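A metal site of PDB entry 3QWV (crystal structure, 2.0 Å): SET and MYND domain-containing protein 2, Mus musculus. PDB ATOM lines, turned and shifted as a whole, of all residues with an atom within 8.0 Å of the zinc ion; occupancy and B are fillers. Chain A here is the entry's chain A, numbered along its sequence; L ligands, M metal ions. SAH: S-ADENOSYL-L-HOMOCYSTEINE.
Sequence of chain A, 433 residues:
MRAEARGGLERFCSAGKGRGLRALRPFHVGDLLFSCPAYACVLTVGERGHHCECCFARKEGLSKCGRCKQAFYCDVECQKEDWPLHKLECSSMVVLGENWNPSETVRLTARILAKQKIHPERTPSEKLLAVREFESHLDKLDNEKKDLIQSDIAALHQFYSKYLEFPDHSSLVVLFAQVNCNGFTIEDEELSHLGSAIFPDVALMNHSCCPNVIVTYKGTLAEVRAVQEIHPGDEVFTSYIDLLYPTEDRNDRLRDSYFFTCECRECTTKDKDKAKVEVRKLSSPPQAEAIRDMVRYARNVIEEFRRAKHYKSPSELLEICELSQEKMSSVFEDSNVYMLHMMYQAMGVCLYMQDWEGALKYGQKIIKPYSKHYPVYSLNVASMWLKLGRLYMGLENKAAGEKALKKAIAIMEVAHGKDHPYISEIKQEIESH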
ATOM      1  N   HIS A 207      16.315 -11.282  27.833  1.00  0.00           N
ATOM      2  CA  HIS A 207      17.728 -10.924  28.014  1.00  0.00           C
ATOM      3  C   HIS A 207      17.922  -9.678  28.865  1.00  0.00           C
ATOM      4  O   HIS A 207      17.146  -8.725  28.785  1.00  0.00           O
ATOM      5  CB  HIS A 207      18.366 -10.660  26.634  1.00  0.00           C
ATOM      6  CG  HIS A 207      19.724 -10.019  26.693  1.00  0.00           C
ATOM      7  ND1 HIS A 207      20.873 -10.780  26.783  1.00  0.00           N
ATOM      8  CD2 HIS A 207      20.062  -8.700  26.740  1.00  0.00           C
ATOM      9  CE1 HIS A 207      21.877  -9.921  26.901  1.00  0.00           C
ATOM     10  NE2 HIS A 207      21.435  -8.647  26.870  1.00  0.00           N
ATOM     11  N   SER A 208      19.060  -9.625  29.568  1.00  0.00           N
ATOM     12  CA  SER A 208      19.656  -8.446  30.205  1.00  0.00           C
ATOM     13  C   SER A 208      21.177  -8.615  30.165  1.00  0.00           C
ATOM     14  O   SER A 208      21.655  -9.734  30.258  1.00  0.00           O
ATOM     15  CB  SER A 208      19.200  -8.273  31.648  1.00  0.00           C
ATOM     16  OG  SER A 208      19.940  -7.229  32.264  1.00  0.00           O
ATOM     17  N   CYS A 209      21.948  -7.501  30.046  1.00  0.00           N
ATOM     18  CA  CYS A 209      23.403  -7.569  30.146  1.00  0.00           C
ATOM     19  C   CYS A 209      23.817  -7.515  31.623  1.00  0.00           C
ATOM     20  O   CYS A 209      25.012  -7.562  31.912  1.00  0.00           O
ATOM     21  CB  CYS A 209      24.073  -6.449  29.340  1.00  0.00           C
ATOM     22  SG  CYS A 209      23.428  -6.263  27.672  1.00  0.00           S
ATOM     23  N   CYS A 210      22.836  -7.394  32.567  1.00  0.00           N
ATOM     24  CA  CYS A 210      23.013  -7.463  34.030  1.00  0.00           C
ATOM     25  C   CYS A 210      22.109  -8.635  34.454  1.00  0.00           C
ATOM     26  O   CYS A 210      21.082  -8.391  35.092  1.00  0.00           O
ATOM     27  CB  CYS A 210      22.587  -6.164  34.712  1.00  0.00           C
ATOM     28  SG  CYS A 210      23.372  -4.675  34.049  1.00  0.00           S
ATOM     29  N   PRO A 211      22.342  -9.877  33.965  1.00  0.00           N
ATOM     30  CA  PRO A 211      21.373 -10.967  34.260  1.00  0.00           C
ATOM     31  C   PRO A 211      21.291 -11.327  35.732  1.00  0.00           C
ATOM     32  O   PRO A 211      22.274 -11.209  36.454  1.00  0.00           O
ATOM     33  CB  PRO A 211      21.910 -12.160  33.423  1.00  0.00           C
ATOM     34  CG  PRO A 211      23.407 -11.884  33.290  1.00  0.00           C
ATOM     35  CD  PRO A 211      23.482 -10.372  33.145  1.00  0.00           C
ATOM     36  N   ILE A 241      24.171 -13.288  25.216  1.00  0.00           N
ATOM     37  CA  ILE A 241      25.432 -13.033  24.513  1.00  0.00           C
ATOM     38  C   ILE A 241      26.626 -12.941  25.438  1.00  0.00           C
ATOM     39  O   ILE A 241      26.474 -12.928  26.662  1.00  0.00           O
ATOM     40  CB  ILE A 241      25.266 -11.703  23.707  1.00  0.00           C
ATOM     41  CG1 ILE A 241      24.787 -10.543  24.651  1.00  0.00           C
ATOM     42  CG2 ILE A 241      24.314 -11.878  22.479  1.00  0.00           C
ATOM     43  CD1 ILE A 241      25.062  -9.197  24.151  1.00  0.00           C
ATOM     44  N   LEU A 243      29.176 -11.031  27.416  1.00  0.00           N
ATOM     45  CA  LEU A 243      29.169  -9.709  28.068  1.00  0.00           C
ATOM     46  C   LEU A 243      30.462  -8.947  28.065  1.00  0.00           C
ATOM     47  O   LEU A 243      30.499  -7.835  28.585  1.00  0.00           O
ATOM     48  CB  LEU A 243      28.573  -9.789  29.493  1.00  0.00           C
ATOM     49  CG  LEU A 243      27.118 -10.346  29.488  1.00  0.00           C
ATOM     50  CD1 LEU A 243      26.597 -10.586  30.902  1.00  0.00           C
ATOM     51  CD2 LEU A 243      26.183  -9.488  28.587  1.00  0.00           C
ATOM     52  N   THR A 247      28.921  -1.614  24.885  1.00  0.00           N
ATOM     53  CA  THR A 247      27.457  -1.526  24.685  1.00  0.00           C
ATOM     54  C   THR A 247      27.011  -1.596  23.217  1.00  0.00           C
ATOM     55  O   THR A 247      26.039  -2.297  22.896  1.00  0.00           O
ATOM     56  CB  THR A 247      26.909  -0.273  25.409  1.00  0.00           C
ATOM     57  OG1 THR A 247      27.244  -0.322  26.799  1.00  0.00           O
ATOM     58  CG2 THR A 247      25.413  -0.098  25.234  1.00  0.00           C
ATOM     59  N   ARG A 250      27.405  -5.095  21.758  1.00  0.00           N
ATOM     60  CA  ARG A 250      26.356  -5.932  22.367  1.00  0.00           C
ATOM     61  C   ARG A 250      25.026  -5.665  21.679  1.00  0.00           C
ATOM     62  O   ARG A 250      24.399  -6.608  21.246  1.00  0.00           O
ATOM     63  CB  ARG A 250      26.255  -5.689  23.897  1.00  0.00           C
ATOM     64  CG  ARG A 250      27.448  -6.172  24.727  1.00  0.00           C
ATOM     65  CD  ARG A 250      27.080  -6.366  26.209  1.00  0.00           C
ATOM     66  NE  ARG A 250      26.330  -5.217  26.756  1.00  0.00           N
ATOM     67  CZ  ARG A 250      26.884  -4.095  27.199  1.00  0.00           C
ATOM     68  NH1 ARG A 250      28.205  -3.928  27.132  1.00  0.00           N
ATOM     69  NH2 ARG A 250      26.128  -3.113  27.678  1.00  0.00           N
ATOM     70  N   ASN A 251      24.638  -4.398  21.523  1.00  0.00           N
ATOM     71  CA  ASN A 251      23.347  -4.057  20.900  1.00  0.00           C
ATOM     72  C   ASN A 251      23.245  -4.349  19.414  1.00  0.00           C
ATOM     73  O   ASN A 251      22.193  -4.794  18.974  1.00  0.00           O
ATOM     74  CB  ASN A 251      22.856  -2.680  21.314  1.00  0.00           C
ATOM     75  CG  ASN A 251      22.120  -2.730  22.635  1.00  0.00           C
ATOM     76  OD1 ASN A 251      21.160  -3.471  22.799  1.00  0.00           O
ATOM     77  ND2 ASN A 251      22.585  -2.026  23.623  1.00  0.00           N
ATOM     78  N   LEU A 254      22.608  -8.067  19.451  1.00  0.00           N
ATOM     79  CA  LEU A 254      21.225  -8.302  19.864  1.00  0.00           C
ATOM     80  C   LEU A 254      20.205  -7.982  18.776  1.00  0.00           C
ATOM     81  O   LEU A 254      19.282  -8.777  18.559  1.00  0.00           O
ATOM     82  CB  LEU A 254      20.862  -7.615  21.198  1.00  0.00           C
ATOM     83  CG  LEU A 254      21.652  -8.133  22.423  1.00  0.00           C
ATOM     84  CD1 LEU A 254      21.504  -7.215  23.627  1.00  0.00           C
ATOM     85  CD2 LEU A 254      21.355  -9.630  22.724  1.00  0.00           C
ATOM     86  N   PHE A 260      15.897  -6.770  18.875  1.00  0.00           N
ATOM     87  CA  PHE A 260      15.543  -5.819  19.944  1.00  0.00           C
ATOM     88  C   PHE A 260      16.794  -5.049  20.362  1.00  0.00           C
ATOM     89  O   PHE A 260      17.901  -5.536  20.157  1.00  0.00           O
ATOM     90  CB  PHE A 260      14.911  -6.543  21.171  1.00  0.00           C
ATOM     91  CG  PHE A 260      15.886  -7.306  22.055  1.00  0.00           C
ATOM     92  CD1 PHE A 260      16.257  -8.609  21.756  1.00  0.00           C
ATOM     93  CD2 PHE A 260      16.447  -6.695  23.189  1.00  0.00           C
ATOM     94  CE1 PHE A 260      17.169  -9.312  22.580  1.00  0.00           C
ATOM     95  CE2 PHE A 260      17.345  -7.407  24.011  1.00  0.00           C
ATOM     96  CZ  PHE A 260      17.716  -8.693  23.687  1.00  0.00           C
ATOM     97  N   THR A 261      16.582  -3.911  21.031  1.00  0.00           N
ATOM     98  CA  THR A 261      17.659  -3.090  21.598  1.00  0.00           C
ATOM     99  C   THR A 261      17.537  -3.211  23.103  1.00  0.00           C
ATOM    100  O   THR A 261      16.466  -2.974  23.651  1.00  0.00           O
ATOM    101  CB  THR A 261      17.543  -1.631  21.104  1.00  0.00           C
ATOM    102  OG1 THR A 261      17.855  -1.644  19.714  1.00  0.00           O
ATOM    103  CG2 THR A 261      18.515  -0.661  21.854  1.00  0.00           C
ATOM    104  N   CYS A 262      18.616  -3.633  23.764  1.00  0.00           N
ATOM    105  CA  CYS A 262      18.591  -3.779  25.201  1.00  0.00           C
ATOM    106  C   CYS A 262      18.568  -2.411  25.894  1.00  0.00           C
ATOM    107  O   CYS A 262      19.286  -1.516  25.481  1.00  0.00           O
ATOM    108  CB  CYS A 262      19.765  -4.620  25.689  1.00  0.00           C
ATOM    109  SG  CYS A 262      19.662  -5.028  27.456  1.00  0.00           S
ATOM    110  N   GLU A 263      17.775  -2.302  26.960  1.00  0.00           N
ATOM    111  CA  GLU A 263      17.652  -1.094  27.781  1.00  0.00           C
ATOM    112  C   GLU A 263      18.020  -1.391  29.248  1.00  0.00           C
ATOM    113  O   GLU A 263      17.629  -0.627  30.139  1.00  0.00           O
ATOM    114  CB  GLU A 263      16.218  -0.526  27.652  1.00  0.00           C
ATOM    115  CG  GLU A 263      15.915   0.037  26.271  1.00  0.00           C
ATOM    116  CD  GLU A 263      14.496   0.559  26.100  1.00  0.00           C
ATOM    117  OE1 GLU A 263      14.081   1.444  26.882  1.00  0.00           O
ATOM    118  OE2 GLU A 263      13.808   0.072  25.176  1.00  0.00           O
ATOM    119  N   CYS A 264      18.821  -2.457  29.518  1.00  0.00           N
ATOM    120  CA  CYS A 264      19.240  -2.777  30.896  1.00  0.00           C
ATOM    121  C   CYS A 264      20.145  -1.634  31.431  1.00  0.00           C
ATOM    122  O   CYS A 264      20.550  -0.740  30.669  1.00  0.00           O
ATOM    123  CB  CYS A 264      19.965  -4.113  30.947  1.00  0.00           C
ATOM    124  SG  CYS A 264      21.686  -4.012  30.386  1.00  0.00           S
ATOM    125  N   ARG A 265      20.478  -1.684  32.718  1.00  0.00           N
ATOM    126  CA  ARG A 265      21.315  -0.684  33.371  1.00  0.00           C
ATOM    127  C   ARG A 265      22.673  -0.483  32.707  1.00  0.00           C
ATOM    128  O   ARG A 265      23.096   0.664  32.527  1.00  0.00           O
ATOM    129  CB  ARG A 265      21.459  -1.049  34.871  1.00  0.00           C
ATOM    130  CG  ARG A 265      22.409  -0.154  35.662  1.00  0.00           C
ATOM    131  CD  ARG A 265      21.684   0.844  36.506  1.00  0.00           C
ATOM    132  NE  ARG A 265      22.643   1.707  37.200  1.00  0.00           N
ATOM    133  CZ  ARG A 265      22.466   3.004  37.395  1.00  0.00           C
ATOM    134  NH1 ARG A 265      21.374   3.602  36.965  1.00  0.00           N
ATOM    135  NH2 ARG A 265      23.394   3.723  38.033  1.00  0.00           N
ATOM    136  N   GLU A 266      23.371  -1.575  32.375  1.00  0.00           N
ATOM    137  CA  GLU A 266      24.668  -1.451  31.706  1.00  0.00           C
ATOM    138  C   GLU A 266      24.551  -0.740  30.345  1.00  0.00           C
ATOM    139  O   GLU A 266      25.360   0.107  30.020  1.00  0.00           O
ATOM    140  CB  GLU A 266      25.404  -2.794  31.598  1.00  0.00           C
ATOM    141  CG  GLU A 266      26.870  -2.670  31.155  1.00  0.00           C
ATOM    142  CD  GLU A 266      27.730  -1.585  31.766  1.00  0.00           C
ATOM    143  OE1 GLU A 266      27.632  -1.365  32.992  1.00  0.00           O
ATOM    144  OE2 GLU A 266      28.530  -0.963  31.027  1.00  0.00           O
ATOM    145  N   CYS A 267      23.514  -1.069  29.585  1.00  0.00           N
ATOM    146  CA  CYS A 267      23.245  -0.450  28.286  1.00  0.00           C
ATOM    147  C   CYS A 267      22.823   1.012  28.419  1.00  0.00           C
ATOM    148  O   CYS A 267      23.021   1.784  27.496  1.00  0.00           O
ATOM    149  CB  CYS A 267      22.196  -1.273  27.527  1.00  0.00           C
ATOM    150  SG  CYS A 267      22.851  -2.813  26.837  1.00  0.00           S
ATOM    151  N   THR A 268      22.224   1.384  29.552  1.00  0.00           N
ATOM    152  CA  THR A 268      21.747   2.751  29.794  1.00  0.00           C
ATOM    153  C   THR A 268      22.897   3.666  30.265  1.00  0.00           C
ATOM    154  O   THR A 268      23.111   4.706  29.679  1.00  0.00           O
ATOM    155  CB  THR A 268      20.580   2.703  30.802  1.00  0.00           C
ATOM    156  OG1 THR A 268      19.531   1.950  30.225  1.00  0.00           O
ATOM    157  CG2 THR A 268      20.080   4.098  31.196  1.00  0.00           C
HETATM  158  N   SAH L   1       9.891 -12.588  25.039  1.00  0.00           N
HETATM  159  CA  SAH L   1      10.154 -13.853  24.172  1.00  0.00           C
HETATM  160  CB  SAH L   1      10.972 -14.827  25.221  1.00  0.00           C
HETATM  161  CG  SAH L   1      12.476 -15.004  24.620  1.00  0.00           C
HETATM  162  SD  SAH L   1      12.904 -15.433  23.114  1.00  0.00           S
HETATM  163  C   SAH L   1       8.747 -14.512  23.818  1.00  0.00           C
HETATM  164  O   SAH L   1       7.690 -13.733  24.057  1.00  0.00           O
HETATM  165  OXT SAH L   1       8.666 -15.628  23.324  1.00  0.00           O
HETATM  166  C5' SAH L   1      13.743 -14.168  22.479  1.00  0.00           C
HETATM  167  C4' SAH L   1      13.016 -12.779  22.076  1.00  0.00           C
HETATM  168  O4' SAH L   1      12.342 -11.996  23.218  1.00  0.00           O
HETATM  169  C3' SAH L   1      13.767 -11.733  21.307  1.00  0.00           C
HETATM  170  O3' SAH L   1      13.901 -12.086  19.997  1.00  0.00           O
HETATM  171  C2' SAH L   1      13.051 -10.450  21.522  1.00  0.00           C
HETATM  172  O2' SAH L   1      11.747 -10.421  20.797  1.00  0.00           O
HETATM  173  C1' SAH L   1      12.541 -10.621  23.018  1.00  0.00           C
HETATM  174  N9  SAH L   1      13.433 -10.094  24.098  1.00  0.00           N
HETATM  175  C8  SAH L   1      14.300 -10.726  24.887  1.00  0.00           C
HETATM  176  N7  SAH L   1      14.870  -9.913  25.748  1.00  0.00           N
HETATM  177  C5  SAH L   1      14.398  -8.716  25.448  1.00  0.00           C
HETATM  178  C6  SAH L   1      14.656  -7.385  26.010  1.00  0.00           C
HETATM  179  N6  SAH L   1      15.565  -7.195  27.065  1.00  0.00           N
HETATM  180  N1  SAH L   1      13.981  -6.290  25.452  1.00  0.00           N
HETATM  181  C2  SAH L   1      13.086  -6.488  24.425  1.00  0.00           C
HETATM  182  N3  SAH L   1      12.762  -7.719  23.804  1.00  0.00           N
HETATM  183  C4  SAH L   1      13.489  -8.772  24.421  1.00  0.00           C
HETATM  184 ZN    ZN M   1      21.841  -4.463  28.089  1.00  0.00          ZN
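N of His 207 is in hydrogen-bond range of N7 of the ligand, at 2.9 Å. The backbone carbonyl oxygen of His 207 sits at hydrogen-bond distance from a nitrogen (N6) of the ligand (2.8 Å).
NH2 of Arg 250 sits close to SG of Cys 267 (3.4 Å). NE of Arg 250 lies close to SG of Cys 209 (3.2 Å). The backbone NH (N) of Glu 266 lies close to the side-chain sulfur (SG) of Cys 264 (3.6 Å). N of Cys 262 lies within hydrogen-bond range of OD1 of Asn 251 (2.7 Å). O of Cys 264 is in hydrogen-bond range of OG1 of Thr 268. The backbone NH (N) of Cys 209 lies within hydrogen-bond range of a ring nitrogen (NE2) of His 207 (3.4 Å). The side-chain sulfur (SG) of Cys 267 lies close to the side-chain amide nitrogen (ND2) of Asn 251 (3.3 Å).
The nearest printed residue that does not touch the zinc ion is His 207 (4.4 Å).
The zinc ion is bound by the side-chain sulfur of Cys 267 (2.3 Å), the side-chain sulfur of Cys 262 (2.3 Å), the side-chain sulfur of Cys 264 (2.3 Å) and the side-chain sulfur of Cys 209 (2.4 Å). The zinc ion has four donor atoms within binding distance.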
